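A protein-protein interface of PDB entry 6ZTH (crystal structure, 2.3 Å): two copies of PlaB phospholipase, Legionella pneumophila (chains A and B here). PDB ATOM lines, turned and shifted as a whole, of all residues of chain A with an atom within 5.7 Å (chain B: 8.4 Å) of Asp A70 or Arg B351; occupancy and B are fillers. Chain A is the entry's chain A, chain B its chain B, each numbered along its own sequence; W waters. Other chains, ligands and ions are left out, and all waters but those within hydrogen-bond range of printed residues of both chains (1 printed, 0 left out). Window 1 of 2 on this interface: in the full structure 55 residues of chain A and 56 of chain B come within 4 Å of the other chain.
Among the printed residues, pairs that only touch across the chains: Asp A71 with Val B463 (3.0 Å), Arg A74 with Arg B461 (3.5 Å), Asp A70 with Arg B351 (3.5 Å), Ala A75 with Val B467 (3.5 Å), Ile A72 with Val B467 (3.6 Å), Ala A75 with Ile B488 (3.7 Å), Arg A74 with Ile B488 (3.7 Å) and Arg A74 with Val B463 (3.9 Å).
OD2 of Asp A71 lies within salt-bridge range of NH1 of Arg B461, 2.5 Å away.
O of Asp B489 lies within salt-bridge range of NH2 of Arg A74 (3.0 Å).
The guanidinium group of Arg A74 sits close to the guanidinium group of Arg B351 (3.0 Å).
The guanidinium group (NH2) of Arg A74 lies close to the side-chain amino group (NZ) of Lys B487.
Asp A70 touches one residue of chain B.
Of the printed residues of chain A, Val B463 touches Asp A71 and Arg A74.
Of the printed residues of chain A, Val B467 touches Ile A72 (3.6 Å) and Ala A75 (3.5 Å).
Printed residues of chain A within 4 Å of Lys B487: Arg A74 (2.9 Å).
The nearest residue of chain B that does not touch Asp A70 is Asn B353 (6.0 Å).
No position is printed for both chains.
Of the 12 pairs that touch across the chains among the printed residues, none has its exchanged pair printed and touching as well.
Printed residues of chain A that touch a printed residue of chain B: Asp A70, Asp A71, Ile A72, Arg A74 and Ala A75.
Of the 19 printed residues of chain B, 7 touch a printed residue of chain A.
Hydrophobic or aromatic side chains of chain B that line the printed part of chain A: Val B463, Val B467 and Ile B488.
Along chain B the printed residues that touch a printed residue of chain A span positions 351 to 489.
The backbone NH (N) of Asp A70 sits close to the side-chain hydroxyl (OG1) of Thr A68.
The backbone NH (N) of Asp A71 sits at hydrogen-bond distance from the side-chain hydroxyl (OG1) of Thr A68 (2.7 Å).
N of Arg B351 is in hydrogen-bond range of OD1 of Asp B349, 2.6 Å away.
The side-chain carboxylate (OD1) of Asp B350 sits at hydrogen-bond distance from the backbone NH (N) of Arg B461.
NZ of Lys B487 is in hydrogen-bond range of O of Arg B461, 3.3 Å away.
The backbone carbonyl oxygen of Val B463 lies within hydrogen-bond range of the backbone NH of Ile B488.
Water W1 lies within hydrogen-bond range of the guanidinium group (NH1) of Arg B351 (2.8 Å) and the side-chain hydroxyl (OH) of Tyr A113 (3.2 Å).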
ATOM      1  N   THR A  68       5.759 -10.312   7.423  1.00  0.00           N
ATOM      2  CA  THR A  68       6.272  -8.985   7.132  1.00  0.00           C
ATOM      3  C   THR A  68       5.626  -7.943   8.044  1.00  0.00           C
ATOM      4  O   THR A  68       4.708  -8.230   8.815  1.00  0.00           O
ATOM      5  CB  THR A  68       6.005  -8.626   5.669  1.00  0.00           C
ATOM      6  OG1 THR A  68       4.592  -8.492   5.467  1.00  0.00           O
ATOM      7  CG2 THR A  68       6.543  -9.703   4.739  1.00  0.00           C
ATOM      8  N   VAL A  69       6.123  -6.709   7.942  1.00  0.00           N
ATOM      9  CA  VAL A  69       5.458  -5.587   8.598  1.00  0.00           C
ATOM     10  C   VAL A  69       4.133  -5.290   7.908  1.00  0.00           C
ATOM     11  O   VAL A  69       3.115  -5.041   8.565  1.00  0.00           O
ATOM     12  CB  VAL A  69       6.388  -4.359   8.614  1.00  0.00           C
ATOM     13  CG1 VAL A  69       5.631  -3.101   9.023  1.00  0.00           C
ATOM     14  CG2 VAL A  69       7.567  -4.606   9.546  1.00  0.00           C
ATOM     15  N   ASP A  70       4.124  -5.315   6.572  1.00  0.00           N
ATOM     16  CA  ASP A  70       2.870  -5.190   5.836  1.00  0.00           C
ATOM     17  C   ASP A  70       1.868  -6.243   6.289  1.00  0.00           C
ATOM     18  O   ASP A  70       0.669  -5.964   6.406  1.00  0.00           O
ATOM     19  CB  ASP A  70       3.136  -5.311   4.333  1.00  0.00           C
ATOM     20  CG  ASP A  70       1.863  -5.271   3.508  1.00  0.00           C
ATOM     21  OD1 ASP A  70       1.210  -4.209   3.460  1.00  0.00           O
ATOM     22  OD2 ASP A  70       1.516  -6.307   2.901  1.00  0.00           O
ATOM     23  N   ASP A  71       2.344  -7.464   6.549  1.00  0.00           N
ATOM     24  CA  ASP A  71       1.458  -8.512   7.046  1.00  0.00           C
ATOM     25  C   ASP A  71       0.827  -8.113   8.374  1.00  0.00           C
ATOM     26  O   ASP A  71      -0.379  -8.293   8.578  1.00  0.00           O
ATOM     27  CB  ASP A  71       2.231  -9.822   7.205  1.00  0.00           C
ATOM     28  CG  ASP A  71       2.526 -10.497   5.878  1.00  0.00           C
ATOM     29  OD1 ASP A  71       1.699 -10.392   4.950  1.00  0.00           O
ATOM     30  OD2 ASP A  71       3.591 -11.138   5.766  1.00  0.00           O
ATOM     31  N   ILE A  72       1.629  -7.563   9.289  1.00  0.00           N
ATOM     32  CA  ILE A  72       1.127  -7.247  10.622  1.00  0.00           C
ATOM     33  C   ILE A  72       0.180  -6.055  10.568  1.00  0.00           C
ATOM     34  O   ILE A  72      -0.882  -6.062  11.201  1.00  0.00           O
ATOM     35  CB  ILE A  72       2.305  -7.002  11.585  1.00  0.00           C
ATOM     36  CG1 ILE A  72       3.123  -8.286  11.753  1.00  0.00           C
ATOM     37  CG2 ILE A  72       1.808  -6.529  12.945  1.00  0.00           C
ATOM     38  CD1 ILE A  72       4.504  -8.073  12.342  1.00  0.00           C
ATOM     39  N   ALA A  73       0.544  -5.011   9.818  1.00  0.00           N
ATOM     40  CA  ALA A  73      -0.350  -3.866   9.669  1.00  0.00           C
ATOM     41  C   ALA A  73      -1.692  -4.296   9.093  1.00  0.00           C
ATOM     42  O   ALA A  73      -2.750  -3.848   9.552  1.00  0.00           O
ATOM     43  CB  ALA A  73       0.297  -2.806   8.779  1.00  0.00           C
ATOM     44  N   ARG A  74      -1.665  -5.161   8.078  1.00  0.00           N
ATOM     45  CA  ARG A  74      -2.895  -5.732   7.542  1.00  0.00           C
ATOM     46  C   ARG A  74      -3.647  -6.511   8.612  1.00  0.00           C
ATOM     47  O   ARG A  74      -4.869  -6.383   8.749  1.00  0.00           O
ATOM     48  CB  ARG A  74      -2.559  -6.637   6.361  1.00  0.00           C
ATOM     49  CG  ARG A  74      -3.709  -6.943   5.436  1.00  0.00           C
ATOM     50  CD  ARG A  74      -3.162  -7.554   4.160  1.00  0.00           C
ATOM     51  NE  ARG A  74      -4.076  -8.513   3.555  1.00  0.00           N
ATOM     52  CZ  ARG A  74      -3.701  -9.665   3.001  1.00  0.00           C
ATOM     53  NH1 ARG A  74      -2.423 -10.022   2.974  1.00  0.00           N
ATOM     54  NH2 ARG A  74      -4.616 -10.461   2.469  1.00  0.00           N
ATOM     55  N   ALA A  75      -2.928  -7.339   9.374  1.00  0.00           N
ATOM     56  CA  ALA A  75      -3.569  -8.119  10.426  1.00  0.00           C
ATOM     57  C   ALA A  75      -4.125  -7.225  11.524  1.00  0.00           C
ATOM     58  O   ALA A  75      -5.127  -7.576  12.159  1.00  0.00           O
ATOM     59  CB  ALA A  75      -2.575  -9.125  11.004  1.00  0.00           C
ATOM     60  N   LYS A 108       2.269   2.394   9.265  1.00  0.00           N
ATOM     61  CA  LYS A 108       2.103   1.668   8.013  1.00  0.00           C
ATOM     62  C   LYS A 108       0.645   1.322   7.758  1.00  0.00           C
ATOM     63  O   LYS A 108       0.218   1.242   6.600  1.00  0.00           O
ATOM     64  CB  LYS A 108       2.953   0.398   8.036  1.00  0.00           C
ATOM     65  CG  LYS A 108       3.040  -0.322   6.702  1.00  0.00           C
ATOM     66  CD  LYS A 108       3.772   0.516   5.666  1.00  0.00           C
ATOM     67  CE  LYS A 108       4.243  -0.337   4.499  1.00  0.00           C
ATOM     68  NZ  LYS A 108       3.153  -0.575   3.513  1.00  0.00           N
ATOM     69  N   LEU A 112      -1.670   2.221   4.445  1.00  0.00           N
ATOM     70  CA  LEU A 112      -2.331   1.235   3.600  1.00  0.00           C
ATOM     71  C   LEU A 112      -3.808   1.551   3.402  1.00  0.00           C
ATOM     72  O   LEU A 112      -4.366   1.251   2.340  1.00  0.00           O
ATOM     73  CB  LEU A 112      -2.187  -0.163   4.205  1.00  0.00           C
ATOM     74  CG  LEU A 112      -0.801  -0.804   4.231  1.00  0.00           C
ATOM     75  CD1 LEU A 112      -0.845  -2.076   5.072  1.00  0.00           C
ATOM     76  CD2 LEU A 112      -0.300  -1.107   2.829  1.00  0.00           C
ATOM     77  N   TYR A 113      -4.456   2.158   4.399  1.00  0.00           N
ATOM     78  CA  TYR A 113      -5.906   2.227   4.424  1.00  0.00           C
ATOM     79  C   TYR A 113      -6.491   3.632   4.408  1.00  0.00           C
ATOM     80  O   TYR A 113      -7.669   3.772   4.058  1.00  0.00           O
ATOM     81  CB  TYR A 113      -6.447   1.493   5.667  1.00  0.00           C
ATOM     82  CG  TYR A 113      -6.274  -0.010   5.615  1.00  0.00           C
ATOM     83  CD1 TYR A 113      -7.253  -0.821   5.056  1.00  0.00           C
ATOM     84  CD2 TYR A 113      -5.133  -0.617   6.123  1.00  0.00           C
ATOM     85  CE1 TYR A 113      -7.100  -2.195   5.004  1.00  0.00           C
ATOM     86  CE2 TYR A 113      -4.971  -1.990   6.074  1.00  0.00           C
ATOM     87  CZ  TYR A 113      -5.958  -2.774   5.514  1.00  0.00           C
ATOM     88  OH  TYR A 113      -5.802  -4.141   5.463  1.00  0.00           O
ATOM     89  N   ILE B 348       4.342 -13.658  -8.889  1.00  0.00           N
ATOM     90  CA  ILE B 348       4.297 -12.626  -7.862  1.00  0.00           C
ATOM     91  C   ILE B 348       3.132 -12.951  -6.939  1.00  0.00           C
ATOM     92  O   ILE B 348       2.509 -14.011  -7.061  1.00  0.00           O
ATOM     93  CB  ILE B 348       4.159 -11.228  -8.486  1.00  0.00           C
ATOM     94  CG1 ILE B 348       2.863 -11.118  -9.287  1.00  0.00           C
ATOM     95  CG2 ILE B 348       5.344 -10.941  -9.398  1.00  0.00           C
ATOM     96  CD1 ILE B 348       2.648  -9.760  -9.930  1.00  0.00           C
ATOM     97  N   ASP B 349       2.831 -12.053  -6.005  1.00  0.00           N
ATOM     98  CA  ASP B 349       1.637 -12.174  -5.182  1.00  0.00           C
ATOM     99  C   ASP B 349       0.921 -10.831  -5.148  1.00  0.00           C
ATOM    100  O   ASP B 349       1.435  -9.810  -5.615  1.00  0.00           O
ATOM    101  CB  ASP B 349       1.964 -12.671  -3.763  1.00  0.00           C
ATOM    102  CG  ASP B 349       2.808 -11.693  -2.962  1.00  0.00           C
ATOM    103  OD1 ASP B 349       2.616 -10.466  -3.087  1.00  0.00           O
ATOM    104  OD2 ASP B 349       3.660 -12.165  -2.180  1.00  0.00           O
ATOM    105  N   ASP B 350      -0.284 -10.843  -4.585  1.00  0.00           N
ATOM    106  CA  ASP B 350      -1.110  -9.646  -4.497  1.00  0.00           C
ATOM    107  C   ASP B 350      -0.542  -8.588  -3.544  1.00  0.00           C
ATOM    108  O   ASP B 350      -1.230  -7.581  -3.331  1.00  0.00           O
ATOM    109  CB  ASP B 350      -2.530 -10.024  -4.061  1.00  0.00           C
ATOM    110  CG  ASP B 350      -2.550 -11.055  -2.943  1.00  0.00           C
ATOM    111  OD1 ASP B 350      -1.502 -11.692  -2.700  1.00  0.00           O
ATOM    112  OD2 ASP B 350      -3.616 -11.236  -2.319  1.00  0.00           O
ATOM    113  N   ARG B 351       0.657  -8.752  -2.980  1.00  0.00           N
ATOM    114  CA  ARG B 351       1.205  -7.792  -2.032  1.00  0.00           C
ATOM    115  C   ARG B 351       2.460  -7.092  -2.536  1.00  0.00           C
ATOM    116  O   ARG B 351       2.982  -6.213  -1.838  1.00  0.00           O
ATOM    117  CB  ARG B 351       1.519  -8.480  -0.697  1.00  0.00           C
ATOM    118  CG  ARG B 351       0.297  -8.984   0.058  1.00  0.00           C
ATOM    119  CD  ARG B 351      -0.590  -7.839   0.530  1.00  0.00           C
ATOM    120  NE  ARG B 351      -2.010  -8.173   0.444  1.00  0.00           N
ATOM    121  CZ  ARG B 351      -2.996  -7.350   0.787  1.00  0.00           C
ATOM    122  NH1 ARG B 351      -2.721  -6.136   1.244  1.00  0.00           N
ATOM    123  NH2 ARG B 351      -4.257  -7.742   0.673  1.00  0.00           N
ATOM    124  N   GLY B 352       2.962  -7.450  -3.715  1.00  0.00           N
ATOM    125  CA  GLY B 352       4.156  -6.859  -4.266  1.00  0.00           C
ATOM    126  C   GLY B 352       5.404  -7.706  -4.122  1.00  0.00           C
ATOM    127  O   GLY B 352       6.390  -7.454  -4.825  1.00  0.00           O
ATOM    128  N   ASN B 353       5.389  -8.697  -3.234  1.00  0.00           N
ATOM    129  CA  ASN B 353       6.546  -9.567  -3.080  1.00  0.00           C
ATOM    130  C   ASN B 353       6.727 -10.425  -4.326  1.00  0.00           C
ATOM    131  O   ASN B 353       5.753 -10.899  -4.921  1.00  0.00           O
ATOM    132  CB  ASN B 353       6.393 -10.469  -1.852  1.00  0.00           C
ATOM    133  CG  ASN B 353       5.770  -9.755  -0.666  1.00  0.00           C
ATOM    134  OD1 ASN B 353       4.928 -10.318   0.037  1.00  0.00           O
ATOM    135  ND2 ASN B 353       6.184  -8.515  -0.432  1.00  0.00           N
ATOM    136  N   HIS B 354       7.981 -10.623  -4.722  1.00  0.00           N
ATOM    137  CA  HIS B 354       8.318 -11.507  -5.831  1.00  0.00           C
ATOM    138  C   HIS B 354       8.641 -12.891  -5.277  1.00  0.00           C
ATOM    139  O   HIS B 354       9.621 -13.059  -4.543  1.00  0.00           O
ATOM    140  CB  HIS B 354       9.501 -10.959  -6.627  1.00  0.00           C
ATOM    141  CG  HIS B 354       9.310  -9.554  -7.109  1.00  0.00           C
ATOM    142  ND1 HIS B 354       9.431  -8.461  -6.280  1.00  0.00           N
ATOM    143  CD2 HIS B 354       9.015  -9.064  -8.337  1.00  0.00           C
ATOM    144  CE1 HIS B 354       9.216  -7.357  -6.974  1.00  0.00           C
ATOM    145  NE2 HIS B 354       8.960  -7.696  -8.224  1.00  0.00           N
ATOM    146  N   LEU B 355       7.817 -13.877  -5.624  1.00  0.00           N
ATOM    147  CA  LEU B 355       8.022 -15.235  -5.139  1.00  0.00           C
ATOM    148  C   LEU B 355       9.313 -15.810  -5.712  1.00  0.00           C
ATOM    149  O   LEU B 355       9.515 -15.813  -6.931  1.00  0.00           O
ATOM    150  CB  LEU B 355       6.837 -16.118  -5.528  1.00  0.00           C
ATOM    151  CG  LEU B 355       5.558 -16.073  -4.687  1.00  0.00           C
ATOM    152  CD1 LEU B 355       5.703 -16.920  -3.426  1.00  0.00           C
ATOM    153  CD2 LEU B 355       5.162 -14.647  -4.331  1.00  0.00           C
ATOM    154  N   TYR B 431       0.851 -19.445   1.036  1.00  0.00           N
ATOM    155  CA  TYR B 431       0.154 -19.462  -0.241  1.00  0.00           C
ATOM    156  C   TYR B 431      -0.502 -20.821  -0.448  1.00  0.00           C
ATOM    157  O   TYR B 431      -0.156 -21.808   0.207  1.00  0.00           O
ATOM    158  CB  TYR B 431       1.113 -19.159  -1.399  1.00  0.00           C
ATOM    159  CG  TYR B 431       1.807 -17.819  -1.285  1.00  0.00           C
ATOM    160  CD1 TYR B 431       1.196 -16.660  -1.742  1.00  0.00           C
ATOM    161  CD2 TYR B 431       3.073 -17.713  -0.720  1.00  0.00           C
ATOM    162  CE1 TYR B 431       1.824 -15.433  -1.643  1.00  0.00           C
ATOM    163  CE2 TYR B 431       3.710 -16.487  -0.615  1.00  0.00           C
ATOM    164  CZ  TYR B 431       3.078 -15.351  -1.080  1.00  0.00           C
ATOM    165  OH  TYR B 431       3.699 -14.128  -0.981  1.00  0.00           O
ATOM    166  N   MET B 458       0.108 -14.733 -10.409  1.00  0.00           N
ATOM    167  CA  MET B 458      -0.084 -13.964  -9.184  1.00  0.00           C
ATOM    168  C   MET B 458      -0.869 -14.754  -8.141  1.00  0.00           C
ATOM    169  O   MET B 458      -2.014 -15.137  -8.375  1.00  0.00           O
ATOM    170  CB  MET B 458      -0.809 -12.652  -9.493  1.00  0.00           C
ATOM    171  CG  MET B 458      -0.830 -11.661  -8.341  1.00  0.00           C
ATOM    172  SD  MET B 458      -1.627  -9.950  -8.838  1.00  0.00           S
ATOM    173  CE  MET B 458      -3.194  -9.986  -7.684  1.00  0.00           C
ATOM    174  N   LEU B 459      -0.254 -14.983  -6.984  1.00  0.00           N
ATOM    175  CA  LEU B 459      -0.868 -15.754  -5.914  1.00  0.00           C
ATOM    176  C   LEU B 459      -1.371 -14.841  -4.801  1.00  0.00           C
ATOM    177  O   LEU B 459      -0.914 -13.708  -4.631  1.00  0.00           O
ATOM    178  CB  LEU B 459       0.124 -16.768  -5.340  1.00  0.00           C
ATOM    179  CG  LEU B 459       0.645 -17.843  -6.293  1.00  0.00           C
ATOM    180  CD1 LEU B 459       1.428 -18.886  -5.513  1.00  0.00           C
ATOM    181  CD2 LEU B 459      -0.484 -18.498  -7.066  1.00  0.00           C
ATOM    182  N   GLN B 460      -2.326 -15.362  -4.033  1.00  0.00           N
ATOM    183  CA  GLN B 460      -2.930 -14.634  -2.922  1.00  0.00           C
ATOM    184  C   GLN B 460      -2.143 -14.933  -1.652  1.00  0.00           C
ATOM    185  O   GLN B 460      -2.205 -16.048  -1.124  1.00  0.00           O
ATOM    186  CB  GLN B 460      -4.394 -15.033  -2.755  1.00  0.00           C
ATOM    187  CG  GLN B 460      -5.391 -14.060  -3.350  1.00  0.00           C
ATOM    188  CD  GLN B 460      -6.825 -14.513  -3.147  1.00  0.00           C
ATOM    189  OE1 GLN B 460      -7.096 -15.408  -2.348  1.00  0.00           O
ATOM    190  NE2 GLN B 460      -7.748 -13.898  -3.874  1.00  0.00           N
ATOM    191  N   ARG B 461      -1.405 -13.942  -1.157  1.00  0.00           N
ATOM    192  CA  ARG B 461      -0.683 -14.109   0.099  1.00  0.00           C
ATOM    193  C   ARG B 461      -1.682 -14.163   1.249  1.00  0.00           C
ATOM    194  O   ARG B 461      -2.423 -13.201   1.483  1.00  0.00           O
ATOM    195  CB  ARG B 461       0.316 -12.976   0.303  1.00  0.00           C
ATOM    196  CG  ARG B 461       1.162 -13.142   1.556  1.00  0.00           C
ATOM    197  CD  ARG B 461       2.407 -12.269   1.526  1.00  0.00           C
ATOM    198  NE  ARG B 461       3.092 -12.253   2.817  1.00  0.00           N
ATOM    199  CZ  ARG B 461       3.795 -13.269   3.310  1.00  0.00           C
ATOM    200  NH1 ARG B 461       4.382 -13.154   4.494  1.00  0.00           N
ATOM    201  NH2 ARG B 461       3.916 -14.398   2.624  1.00  0.00           N
ATOM    202  N   ARG B 462      -1.706 -15.284   1.964  1.00  0.00           N
ATOM    203  CA  ARG B 462      -2.713 -15.551   2.986  1.00  0.00           C
ATOM    204  C   ARG B 462      -2.084 -15.398   4.364  1.00  0.00           C
ATOM    205  O   ARG B 462      -1.254 -16.219   4.771  1.00  0.00           O
ATOM    206  CB  ARG B 462      -3.307 -16.946   2.799  1.00  0.00           C
ATOM    207  CG  ARG B 462      -4.038 -17.118   1.476  1.00  0.00           C
ATOM    208  CD  ARG B 462      -4.573 -18.530   1.293  1.00  0.00           C
ATOM    209  NE  ARG B 462      -5.425 -18.946   2.402  1.00  0.00           N
ATOM    210  CZ  ARG B 462      -6.650 -19.455   2.273  1.00  0.00           C
ATOM    211  NH1 ARG B 462      -7.335 -19.803   3.353  1.00  0.00           N
ATOM    212  NH2 ARG B 462      -7.197 -19.616   1.077  1.00  0.00           N
ATOM    213  N   VAL B 463      -2.489 -14.347   5.078  1.00  0.00           N
ATOM    214  CA  VAL B 463      -2.071 -14.099   6.453  1.00  0.00           C
ATOM    215  C   VAL B 463      -3.186 -14.540   7.389  1.00  0.00           C
ATOM    216  O   VAL B 463      -4.366 -14.247   7.153  1.00  0.00           O
ATOM    217  CB  VAL B 463      -1.732 -12.612   6.673  1.00  0.00           C
ATOM    218  CG1 VAL B 463      -1.347 -12.369   8.123  1.00  0.00           C
ATOM    219  CG2 VAL B 463      -0.623 -12.178   5.736  1.00  0.00           C
ATOM    220  N   VAL B 467      -1.691 -13.316  13.406  1.00  0.00           N
ATOM    221  CA  VAL B 467      -0.592 -12.366  13.268  1.00  0.00           C
ATOM    222  C   VAL B 467      -0.886 -11.089  14.043  1.00  0.00           C
ATOM    223  O   VAL B 467       0.038 -10.402  14.493  1.00  0.00           O
ATOM    224  CB  VAL B 467      -0.319 -12.078  11.777  1.00  0.00           C
ATOM    225  CG1 VAL B 467       0.487 -10.801  11.614  1.00  0.00           C
ATOM    226  CG2 VAL B 467       0.408 -13.253  11.139  1.00  0.00           C
ATOM    227  N   LYS B 487      -8.177 -16.883   7.543  1.00  0.00           N
ATOM    228  CA  LYS B 487      -7.451 -15.829   6.856  1.00  0.00           C
ATOM    229  C   LYS B 487      -8.032 -14.457   7.196  1.00  0.00           C
ATOM    230  O   LYS B 487      -9.165 -14.333   7.671  1.00  0.00           O
ATOM    231  CB  LYS B 487      -7.501 -16.061   5.345  1.00  0.00           C
ATOM    232  CG  LYS B 487      -6.384 -15.398   4.562  1.00  0.00           C
ATOM    233  CD  LYS B 487      -6.922 -14.755   3.287  1.00  0.00           C
ATOM    234  CE  LYS B 487      -5.873 -13.906   2.570  1.00  0.00           C
ATOM    235  NZ  LYS B 487      -4.987 -13.140   3.494  1.00  0.00           N
ATOM    236  N   ILE B 488      -7.233 -13.420   6.950  1.00  0.00           N
ATOM    237  CA  ILE B 488      -7.672 -12.041   7.106  1.00  0.00           C
ATOM    238  C   ILE B 488      -8.084 -11.510   5.738  1.00  0.00           C
ATOM    239  O   ILE B 488      -7.666 -12.014   4.692  1.00  0.00           O
ATOM    240  CB  ILE B 488      -6.578 -11.144   7.739  1.00  0.00           C
ATOM    241  CG1 ILE B 488      -5.407 -10.953   6.771  1.00  0.00           C
ATOM    242  CG2 ILE B 488      -6.102 -11.735   9.059  1.00  0.00           C
ATOM    243  CD1 ILE B 488      -4.267 -10.117   7.330  1.00  0.00           C
ATOM    244  N   ASP B 489      -8.911 -10.467   5.744  1.00  0.00           N
ATOM    245  CA  ASP B 489      -9.336  -9.827   4.502  1.00  0.00           C
ATOM    246  C   ASP B 489      -8.181  -9.055   3.871  1.00  0.00           C
ATOM    247  O   ASP B 489      -7.019  -9.452   3.961  1.00  0.00           O
ATOM    248  CB  ASP B 489     -10.515  -8.881   4.742  1.00  0.00           C
ATOM    249  CG  ASP B 489     -11.688  -9.567   5.407  1.00  0.00           C
ATOM    250  OD1 ASP B 489     -11.744 -10.814   5.377  1.00  0.00           O
ATOM    251  OD2 ASP B 489     -12.555  -8.858   5.961  1.00  0.00           O
ATOM    252  OXT ASP B 489      -8.386  -8.008   3.255  1.00  0.00           O
HETATM  253  O   HOH W   1      -3.815  -4.102   2.907  1.00  0.00           O
